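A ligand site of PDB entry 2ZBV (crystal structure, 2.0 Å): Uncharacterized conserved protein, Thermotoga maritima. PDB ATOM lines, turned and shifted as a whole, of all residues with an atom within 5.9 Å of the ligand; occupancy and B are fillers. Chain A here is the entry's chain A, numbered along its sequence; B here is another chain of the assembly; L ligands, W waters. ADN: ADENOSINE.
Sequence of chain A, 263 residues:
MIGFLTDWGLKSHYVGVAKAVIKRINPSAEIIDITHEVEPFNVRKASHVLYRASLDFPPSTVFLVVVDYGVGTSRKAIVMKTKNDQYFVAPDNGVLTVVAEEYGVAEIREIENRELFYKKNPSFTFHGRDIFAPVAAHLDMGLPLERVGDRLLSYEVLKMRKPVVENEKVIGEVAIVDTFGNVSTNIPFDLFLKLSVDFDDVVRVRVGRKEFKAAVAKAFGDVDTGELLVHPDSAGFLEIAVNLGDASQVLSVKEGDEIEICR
A nitrogen (N6) of the ligand sits at hydrogen-bond distance from the backbone carbonyl oxygen (O) of Val 242 of chain B. The backbone carbonyl oxygen of Val 66 sits at hydrogen-bond distance from an oxygen (O3') of the ligand (3.3 Å). NE1 of Trp 8 is in hydrogen-bond range of O3' of the ligand (3.5 Å). The backbone NH (N) of Asp 68 lies within hydrogen-bond range of an oxygen (O3') of the ligand. An oxygen (O5') of the ligand is in hydrogen-bond range of the backbone carbonyl oxygen of Thr 125, 2.7 Å away. An oxygen (O2') of the ligand lies within hydrogen-bond range of the side-chain carboxylate of Asp 7 (2.8 Å). The side-chain amide oxygen (OD1) of Asn 182 of chain B is in hydrogen-bond range of a nitrogen (N6) of the ligand (3.0 Å). N1 of the ligand is in hydrogen-bond range of N of Leu 244 of chain B, at 2.9 Å.
O of Val 66 is in hydrogen-bond range of NE1 of Trp 8. The side-chain carboxylate of Asp 68 is in hydrogen-bond range of the backbone NH of Val 71, 3.3 Å away. The backbone NH of Phe 180 of chain B lies within hydrogen-bond range of the side-chain carboxylate of Asp 178 of chain B. The side-chain carboxylate (OD1) of Asp 178 of chain B is in hydrogen-bond range of the backbone NH (N) of Asn 182 of chain B. OD1 of Asn 243 of chain B sits close to O of Phe 220 of chain B (3.3 Å). The side-chain hydroxyl of Thr 6 is in hydrogen-bond range of the backbone NH of Trp 8. The side-chain carboxylate (OD2) of Asp 7 is in hydrogen-bond range of the backbone NH (N) of Phe 41 (2.9 Å).
Phe 41 touches the ligand (CE1 to C4, 3.4 Å). Val 67 touches the ligand. CA of Tyr 69 touches N3 of the ligand, 3.4 Å away. Val 71 touches the ligand. Phe 126 touches the ligand (CA to O5', 3.5 Å). CD2 of Phe 180 of chain B touches C8 of the ligand, 3.5 Å away. CD2 of Phe 220 of chain B touches C4 of the ligand (3.5 Å). Asn 243 of chain B touches the ligand (C to N1, 3.8 Å). O of Gly 245 of chain B touches N6 of the ligand (3.9 Å). 17 residues have an atom within 4 Å of the ligand: Asp 7, Trp 8, Phe 41, Val 66, Val 67, Asp 68, Tyr 69, Val 71, Thr 125, Phe 126, Phe 180 of chain B, Asn 182 of chain B, Phe 220 of chain B, Val 242 of chain B, Asn 243 of chain B, Leu 244 of chain B and Gly 245 of chain B. The nearest printed residue that does not touch the ligand is Ala 241 of chain B (4.1 Å).
Water W1 lies within hydrogen-bond range of O5' of the ligand, N of Gly 128, OD2 of Asp 68 and N of His 127.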
ATOM      1  N   THR A   6      10.798 -19.461   7.928  1.00  0.00           N
ATOM      2  CA  THR A   6      10.112 -19.941   6.723  1.00  0.00           C
ATOM      3  C   THR A   6       8.687 -19.407   6.607  1.00  0.00           C
ATOM      4  O   THR A   6       8.203 -18.685   7.484  1.00  0.00           O
ATOM      5  CB  THR A   6       9.964 -21.492   6.698  1.00  0.00           C
ATOM      6  OG1 THR A   6       8.889 -21.869   7.556  1.00  0.00           O
ATOM      7  CG2 THR A   6      11.255 -22.200   7.173  1.00  0.00           C
ATOM      8  N   ASP A   7       8.006 -19.798   5.533  1.00  0.00           N
ATOM      9  CA  ASP A   7       6.617 -19.434   5.291  1.00  0.00           C
ATOM     10  C   ASP A   7       5.806 -20.741   5.264  1.00  0.00           C
ATOM     11  O   ASP A   7       4.720 -20.795   4.708  1.00  0.00           O
ATOM     12  CB  ASP A   7       6.470 -18.696   3.943  1.00  0.00           C
ATOM     13  CG  ASP A   7       6.886 -19.564   2.739  1.00  0.00           C
ATOM     14  OD1 ASP A   7       7.650 -20.540   2.936  1.00  0.00           O
ATOM     15  OD2 ASP A   7       6.477 -19.268   1.597  1.00  0.00           O
ATOM     16  N   TRP A   8       6.352 -21.784   5.901  1.00  0.00           N
ATOM     17  CA  TRP A   8       5.703 -23.093   5.904  1.00  0.00           C
ATOM     18  C   TRP A   8       4.496 -23.250   6.822  1.00  0.00           C
ATOM     19  O   TRP A   8       3.633 -24.074   6.562  1.00  0.00           O
ATOM     20  CB  TRP A   8       6.708 -24.196   6.231  1.00  0.00           C
ATOM     21  CG  TRP A   8       7.942 -24.234   5.362  1.00  0.00           C
ATOM     22  CD1 TRP A   8       8.206 -23.464   4.264  1.00  0.00           C
ATOM     23  CD2 TRP A   8       9.122 -25.003   5.607  1.00  0.00           C
ATOM     24  NE1 TRP A   8       9.479 -23.699   3.820  1.00  0.00           N
ATOM     25  CE2 TRP A   8      10.071 -24.636   4.623  1.00  0.00           C
ATOM     26  CE3 TRP A   8       9.473 -25.964   6.572  1.00  0.00           C
ATOM     27  CZ2 TRP A   8      11.351 -25.198   4.578  1.00  0.00           C
ATOM     28  CZ3 TRP A   8      10.758 -26.523   6.519  1.00  0.00           C
ATOM     29  CH2 TRP A   8      11.672 -26.134   5.533  1.00  0.00           C
ATOM     30  N   PRO A  40       2.669 -16.756   2.871  1.00  0.00           N
ATOM     31  CA  PRO A  40       3.141 -17.522   1.711  1.00  0.00           C
ATOM     32  C   PRO A  40       3.868 -16.694   0.640  1.00  0.00           C
ATOM     33  O   PRO A  40       3.365 -15.673   0.189  1.00  0.00           O
ATOM     34  CB  PRO A  40       1.853 -18.143   1.181  1.00  0.00           C
ATOM     35  CG  PRO A  40       1.091 -18.428   2.454  1.00  0.00           C
ATOM     36  CD  PRO A  40       1.308 -17.148   3.250  1.00  0.00           C
ATOM     37  N   PHE A  41       5.051 -17.160   0.265  1.00  0.00           N
ATOM     38  CA  PHE A  41       5.889 -16.554  -0.765  1.00  0.00           C
ATOM     39  C   PHE A  41       6.344 -15.118  -0.497  1.00  0.00           C
ATOM     40  O   PHE A  41       6.976 -14.510  -1.370  1.00  0.00           O
ATOM     41  CB  PHE A  41       5.170 -16.580  -2.127  1.00  0.00           C
ATOM     42  CG  PHE A  41       4.122 -17.662  -2.252  1.00  0.00           C
ATOM     43  CD1 PHE A  41       4.432 -19.001  -2.005  1.00  0.00           C
ATOM     44  CD2 PHE A  41       2.806 -17.343  -2.593  1.00  0.00           C
ATOM     45  CE1 PHE A  41       3.465 -19.987  -2.097  1.00  0.00           C
ATOM     46  CE2 PHE A  41       1.823 -18.333  -2.685  1.00  0.00           C
ATOM     47  CZ  PHE A  41       2.154 -19.660  -2.432  1.00  0.00           C
ATOM     48  N   VAL A  66      14.015 -20.226   4.467  1.00  0.00           N
ATOM     49  CA  VAL A  66      13.344 -20.809   3.328  1.00  0.00           C
ATOM     50  C   VAL A  66      11.938 -20.311   3.018  1.00  0.00           C
ATOM     51  O   VAL A  66      10.937 -20.807   3.540  1.00  0.00           O
ATOM     52  CB  VAL A  66      13.289 -22.362   3.467  1.00  0.00           C
ATOM     53  CG1 VAL A  66      12.778 -22.974   2.167  1.00  0.00           C
ATOM     54  CG2 VAL A  66      14.673 -22.916   3.790  1.00  0.00           C
ATOM     55  N   VAL A  67      11.897 -19.286   2.160  1.00  0.00           N
ATOM     56  CA  VAL A  67      10.661 -18.693   1.635  1.00  0.00           C
ATOM     57  C   VAL A  67      11.137 -18.826   0.192  1.00  0.00           C
ATOM     58  O   VAL A  67      11.859 -17.974  -0.335  1.00  0.00           O
ATOM     59  CB  VAL A  67      10.503 -17.229   2.030  1.00  0.00           C
ATOM     60  CG1 VAL A  67       9.207 -16.673   1.435  1.00  0.00           C
ATOM     61  CG2 VAL A  67      10.466 -17.111   3.554  1.00  0.00           C
ATOM     62  N   ASP A  68      10.725 -19.924  -0.437  1.00  0.00           N
ATOM     63  CA  ASP A  68      11.233 -20.278  -1.751  1.00  0.00           C
ATOM     64  C   ASP A  68      10.193 -20.649  -2.812  1.00  0.00           C
ATOM     65  O   ASP A  68      10.064 -21.820  -3.181  1.00  0.00           O
ATOM     66  CB  ASP A  68      12.215 -21.427  -1.472  1.00  0.00           C
ATOM     67  CG  ASP A  68      13.023 -21.838  -2.661  1.00  0.00           C
ATOM     68  OD1 ASP A  68      13.169 -21.041  -3.608  1.00  0.00           O
ATOM     69  OD2 ASP A  68      13.552 -22.977  -2.603  1.00  0.00           O
ATOM     70  N   TYR A  69       9.474 -19.661  -3.332  1.00  0.00           N
ATOM     71  CA  TYR A  69       8.451 -19.943  -4.343  1.00  0.00           C
ATOM     72  C   TYR A  69       9.058 -20.510  -5.633  1.00  0.00           C
ATOM     73  O   TYR A  69       8.370 -21.170  -6.407  1.00  0.00           O
ATOM     74  CB  TYR A  69       7.664 -18.668  -4.668  1.00  0.00           C
ATOM     75  CG  TYR A  69       8.543 -17.534  -5.183  1.00  0.00           C
ATOM     76  CD1 TYR A  69       8.849 -17.419  -6.541  1.00  0.00           C
ATOM     77  CD2 TYR A  69       9.097 -16.606  -4.304  1.00  0.00           C
ATOM     78  CE1 TYR A  69       9.682 -16.407  -7.013  1.00  0.00           C
ATOM     79  CE2 TYR A  69       9.929 -15.591  -4.762  1.00  0.00           C
ATOM     80  CZ  TYR A  69      10.229 -15.495  -6.107  1.00  0.00           C
ATOM     81  OH  TYR A  69      11.078 -14.501  -6.551  1.00  0.00           O
ATOM     82  N   GLY A  70      10.340 -20.239  -5.861  1.00  0.00           N
ATOM     83  CA  GLY A  70      10.997 -20.731  -7.072  1.00  0.00           C
ATOM     84  C   GLY A  70      11.687 -22.059  -6.874  1.00  0.00           C
ATOM     85  O   GLY A  70      12.550 -22.459  -7.664  1.00  0.00           O
ATOM     86  N   VAL A  71      11.316 -22.760  -5.804  1.00  0.00           N
ATOM     87  CA  VAL A  71      11.903 -24.045  -5.503  1.00  0.00           C
ATOM     88  C   VAL A  71      11.801 -24.962  -6.741  1.00  0.00           C
ATOM     89  O   VAL A  71      10.759 -25.042  -7.382  1.00  0.00           O
ATOM     90  CB  VAL A  71      11.197 -24.713  -4.296  1.00  0.00           C
ATOM     91  CG1 VAL A  71       9.732 -25.022  -4.641  1.00  0.00           C
ATOM     92  CG2 VAL A  71      11.937 -25.974  -3.869  1.00  0.00           C
ATOM     93  N   THR A 125      10.120 -29.988  -5.089  1.00  0.00           N
ATOM     94  CA  THR A 125       9.524 -28.832  -4.429  1.00  0.00           C
ATOM     95  C   THR A 125       9.748 -28.661  -2.925  1.00  0.00           C
ATOM     96  O   THR A 125       9.050 -27.883  -2.282  1.00  0.00           O
ATOM     97  CB  THR A 125       8.002 -28.795  -4.712  1.00  0.00           C
ATOM     98  OG1 THR A 125       7.393 -29.999  -4.226  1.00  0.00           O
ATOM     99  CG2 THR A 125       7.751 -28.688  -6.214  1.00  0.00           C
ATOM    100  N   PHE A 126      10.722 -29.376  -2.346  1.00  0.00           N
ATOM    101  CA  PHE A 126      10.997 -29.233  -0.910  1.00  0.00           C
ATOM    102  C   PHE A 126      12.507 -29.225  -0.640  1.00  0.00           C
ATOM    103  O   PHE A 126      13.008 -30.038   0.143  1.00  0.00           O
ATOM    104  CB  PHE A 126      10.318 -30.355  -0.114  1.00  0.00           C
ATOM    105  CG  PHE A 126      10.175 -30.058   1.366  1.00  0.00           C
ATOM    106  CD1 PHE A 126      10.435 -28.784   1.881  1.00  0.00           C
ATOM    107  CD2 PHE A 126       9.763 -31.045   2.246  1.00  0.00           C
ATOM    108  CE1 PHE A 126      10.286 -28.504   3.248  1.00  0.00           C
ATOM    109  CE2 PHE A 126       9.604 -30.793   3.619  1.00  0.00           C
ATOM    110  CZ  PHE A 126       9.874 -29.512   4.119  1.00  0.00           C
ATOM    111  N   HIS A 127      13.217 -28.321  -1.293  1.00  0.00           N
ATOM    112  CA  HIS A 127      14.657 -28.199  -1.098  1.00  0.00           C
ATOM    113  C   HIS A 127      14.936 -27.802   0.350  1.00  0.00           C
ATOM    114  O   HIS A 127      16.013 -28.047   0.884  1.00  0.00           O
ATOM    115  CB  HIS A 127      15.245 -27.173  -2.059  1.00  0.00           C
ATOM    116  CG  HIS A 127      15.321 -27.646  -3.483  1.00  0.00           C
ATOM    117  ND1 HIS A 127      14.818 -28.869  -3.895  1.00  0.00           N
ATOM    118  CD2 HIS A 127      15.825 -27.058  -4.591  1.00  0.00           C
ATOM    119  CE1 HIS A 127      15.011 -29.003  -5.194  1.00  0.00           C
ATOM    120  NE2 HIS A 127      15.624 -27.928  -5.645  1.00  0.00           N
ATOM    121  N   GLY A 128      13.942 -27.191   1.004  1.00  0.00           N
ATOM    122  CA  GLY A 128      14.106 -26.810   2.395  1.00  0.00           C
ATOM    123  C   GLY A 128      14.519 -27.997   3.250  1.00  0.00           C
ATOM    124  O   GLY A 128      15.346 -27.869   4.152  1.00  0.00           O
ATOM    125  N   ASP B 178      -2.453 -28.108   2.651  1.00  0.00           N
ATOM    126  CA  ASP B 178      -1.485 -27.431   3.505  1.00  0.00           C
ATOM    127  C   ASP B 178      -1.713 -25.931   3.626  1.00  0.00           C
ATOM    128  O   ASP B 178      -2.709 -25.409   3.127  1.00  0.00           O
ATOM    129  CB  ASP B 178      -0.045 -27.733   3.028  1.00  0.00           C
ATOM    130  CG  ASP B 178       0.287 -27.087   1.690  1.00  0.00           C
ATOM    131  OD1 ASP B 178      -0.441 -26.181   1.243  1.00  0.00           O
ATOM    132  OD2 ASP B 178       1.317 -27.474   1.081  1.00  0.00           O
ATOM    133  N   PHE B 180      -0.327 -23.494   2.191  1.00  0.00           N
ATOM    134  CA  PHE B 180      -0.321 -22.771   0.912  1.00  0.00           C
ATOM    135  C   PHE B 180      -1.618 -23.006   0.135  1.00  0.00           C
ATOM    136  O   PHE B 180      -1.921 -22.272  -0.807  1.00  0.00           O
ATOM    137  CB  PHE B 180       0.864 -23.235   0.066  1.00  0.00           C
ATOM    138  CG  PHE B 180       2.183 -23.076   0.747  1.00  0.00           C
ATOM    139  CD1 PHE B 180       2.740 -21.815   0.955  1.00  0.00           C
ATOM    140  CD2 PHE B 180       2.864 -24.188   1.239  1.00  0.00           C
ATOM    141  CE1 PHE B 180       3.943 -21.670   1.630  1.00  0.00           C
ATOM    142  CE2 PHE B 180       4.075 -24.048   1.916  1.00  0.00           C
ATOM    143  CZ  PHE B 180       4.612 -22.783   2.113  1.00  0.00           C
ATOM    144  N   ASN B 182      -2.146 -25.978  -1.162  1.00  0.00           N
ATOM    145  CA  ASN B 182      -1.815 -27.040  -2.086  1.00  0.00           C
ATOM    146  C   ASN B 182      -2.700 -28.212  -1.693  1.00  0.00           C
ATOM    147  O   ASN B 182      -2.954 -28.443  -0.505  1.00  0.00           O
ATOM    148  CB  ASN B 182      -0.340 -27.424  -1.999  1.00  0.00           C
ATOM    149  CG  ASN B 182       0.579 -26.252  -2.330  1.00  0.00           C
ATOM    150  OD1 ASN B 182       0.334 -25.510  -3.269  1.00  0.00           O
ATOM    151  ND2 ASN B 182       1.642 -26.105  -1.544  1.00  0.00           N
ATOM    152  N   PHE B 220       6.695 -25.566  -9.070  1.00  0.00           N
ATOM    153  CA  PHE B 220       5.570 -24.640  -9.132  1.00  0.00           C
ATOM    154  C   PHE B 220       5.840 -23.619 -10.232  1.00  0.00           C
ATOM    155  O   PHE B 220       4.945 -23.256 -11.002  1.00  0.00           O
ATOM    156  CB  PHE B 220       5.417 -23.891  -7.805  1.00  0.00           C
ATOM    157  CG  PHE B 220       5.276 -24.796  -6.607  1.00  0.00           C
ATOM    158  CD1 PHE B 220       4.114 -25.539  -6.416  1.00  0.00           C
ATOM    159  CD2 PHE B 220       6.312 -24.915  -5.699  1.00  0.00           C
ATOM    160  CE1 PHE B 220       3.998 -26.393  -5.332  1.00  0.00           C
ATOM    161  CE2 PHE B 220       6.208 -25.768  -4.608  1.00  0.00           C
ATOM    162  CZ  PHE B 220       5.045 -26.511  -4.416  1.00  0.00           C
ATOM    163  N   GLY B 221       7.095 -23.167 -10.284  1.00  0.00           N
ATOM    164  CA  GLY B 221       7.501 -22.177 -11.268  1.00  0.00           C
ATOM    165  C   GLY B 221       7.580 -22.637 -12.709  1.00  0.00           C
ATOM    166  O   GLY B 221       7.925 -21.848 -13.592  1.00  0.00           O
ATOM    167  N   ALA B 241      -1.515 -27.947  -7.248  1.00  0.00           N
ATOM    168  CA  ALA B 241      -1.156 -26.642  -6.718  1.00  0.00           C
ATOM    169  C   ALA B 241      -1.352 -25.542  -7.735  1.00  0.00           C
ATOM    170  O   ALA B 241      -1.395 -25.786  -8.946  1.00  0.00           O
ATOM    171  CB  ALA B 241       0.307 -26.650  -6.257  1.00  0.00           C
ATOM    172  N   VAL B 242      -1.473 -24.317  -7.227  1.00  0.00           N
ATOM    173  CA  VAL B 242      -1.574 -23.155  -8.091  1.00  0.00           C
ATOM    174  C   VAL B 242      -0.249 -22.451  -7.845  1.00  0.00           C
ATOM    175  O   VAL B 242       0.104 -22.176  -6.695  1.00  0.00           O
ATOM    176  CB  VAL B 242      -2.712 -22.211  -7.681  1.00  0.00           C
ATOM    177  CG1 VAL B 242      -2.591 -20.905  -8.461  1.00  0.00           C
ATOM    178  CG2 VAL B 242      -4.056 -22.867  -7.957  1.00  0.00           C
ATOM    179  N   ASN B 243       0.478 -22.161  -8.909  1.00  0.00           N
ATOM    180  CA  ASN B 243       1.759 -21.487  -8.769  1.00  0.00           C
ATOM    181  C   ASN B 243       1.533 -20.121  -8.155  1.00  0.00           C
ATOM    182  O   ASN B 243       0.853 -19.277  -8.750  1.00  0.00           O
ATOM    183  CB  ASN B 243       2.458 -21.362 -10.130  1.00  0.00           C
ATOM    184  CG  ASN B 243       3.736 -20.537 -10.053  1.00  0.00           C
ATOM    185  OD1 ASN B 243       4.453 -20.586  -9.047  1.00  0.00           O
ATOM    186  ND2 ASN B 243       4.036 -19.810 -11.122  1.00  0.00           N
ATOM    187  N   LEU B 244       2.095 -19.918  -6.974  1.00  0.00           N
ATOM    188  CA  LEU B 244       1.951 -18.644  -6.268  1.00  0.00           C
ATOM    189  C   LEU B 244       0.489 -18.385  -5.914  1.00  0.00           C
ATOM    190  O   LEU B 244       0.067 -17.235  -5.781  1.00  0.00           O
ATOM    191  CB  LEU B 244       2.508 -17.506  -7.138  1.00  0.00           C
ATOM    192  CG  LEU B 244       4.016 -17.565  -7.373  1.00  0.00           C
ATOM    193  CD1 LEU B 244       4.437 -16.512  -8.409  1.00  0.00           C
ATOM    194  CD2 LEU B 244       4.732 -17.343  -6.043  1.00  0.00           C
ATOM    195  N   GLY B 245      -0.279 -19.460  -5.772  1.00  0.00           N
ATOM    196  CA  GLY B 245      -1.690 -19.325  -5.439  1.00  0.00           C
ATOM    197  C   GLY B 245      -2.185 -20.385  -4.481  1.00  0.00           C
ATOM    198  O   GLY B 245      -1.402 -21.123  -3.898  1.00  0.00           O
HETATM  199  O5' ADN L   1       9.966 -25.918  -0.681  1.00  0.00           O
HETATM  200  C5' ADN L   1       9.342 -25.036   0.250  1.00  0.00           C
HETATM  201  C4' ADN L   1       8.841 -23.797  -0.488  1.00  0.00           C
HETATM  202  O4' ADN L   1       7.826 -24.131  -1.491  1.00  0.00           O
HETATM  203  C3' ADN L   1       8.169 -22.757   0.454  1.00  0.00           C
HETATM  204  O3' ADN L   1       9.131 -21.825   0.929  1.00  0.00           O
HETATM  205  C2' ADN L   1       7.081 -22.127  -0.444  1.00  0.00           C
HETATM  206  O2' ADN L   1       7.303 -20.728  -0.629  1.00  0.00           O
HETATM  207  C1' ADN L   1       7.147 -22.885  -1.769  1.00  0.00           C
HETATM  208  N9  ADN L   1       5.785 -23.142  -2.266  1.00  0.00           N
HETATM  209  C8  ADN L   1       4.850 -23.980  -1.696  1.00  0.00           C
HETATM  210  N7  ADN L   1       3.744 -23.975  -2.381  1.00  0.00           N
HETATM  211  C5  ADN L   1       3.888 -23.138  -3.427  1.00  0.00           C
HETATM  212  C6  ADN L   1       3.047 -22.728  -4.500  1.00  0.00           C
HETATM  213  N6  ADN L   1       1.751 -23.215  -4.619  1.00  0.00           N
HETATM  214  N1  ADN L   1       3.532 -21.837  -5.398  1.00  0.00           N
HETATM  215  C2  ADN L   1       4.786 -21.346  -5.306  1.00  0.00           C
HETATM  216  N3  ADN L   1       5.607 -21.717  -4.319  1.00  0.00           N
HETATM  217  C4  ADN L   1       5.200 -22.592  -3.375  1.00  0.00           C
HETATM  218  O   HOH W   1      12.588 -25.175  -0.627  1.00  0.00           O
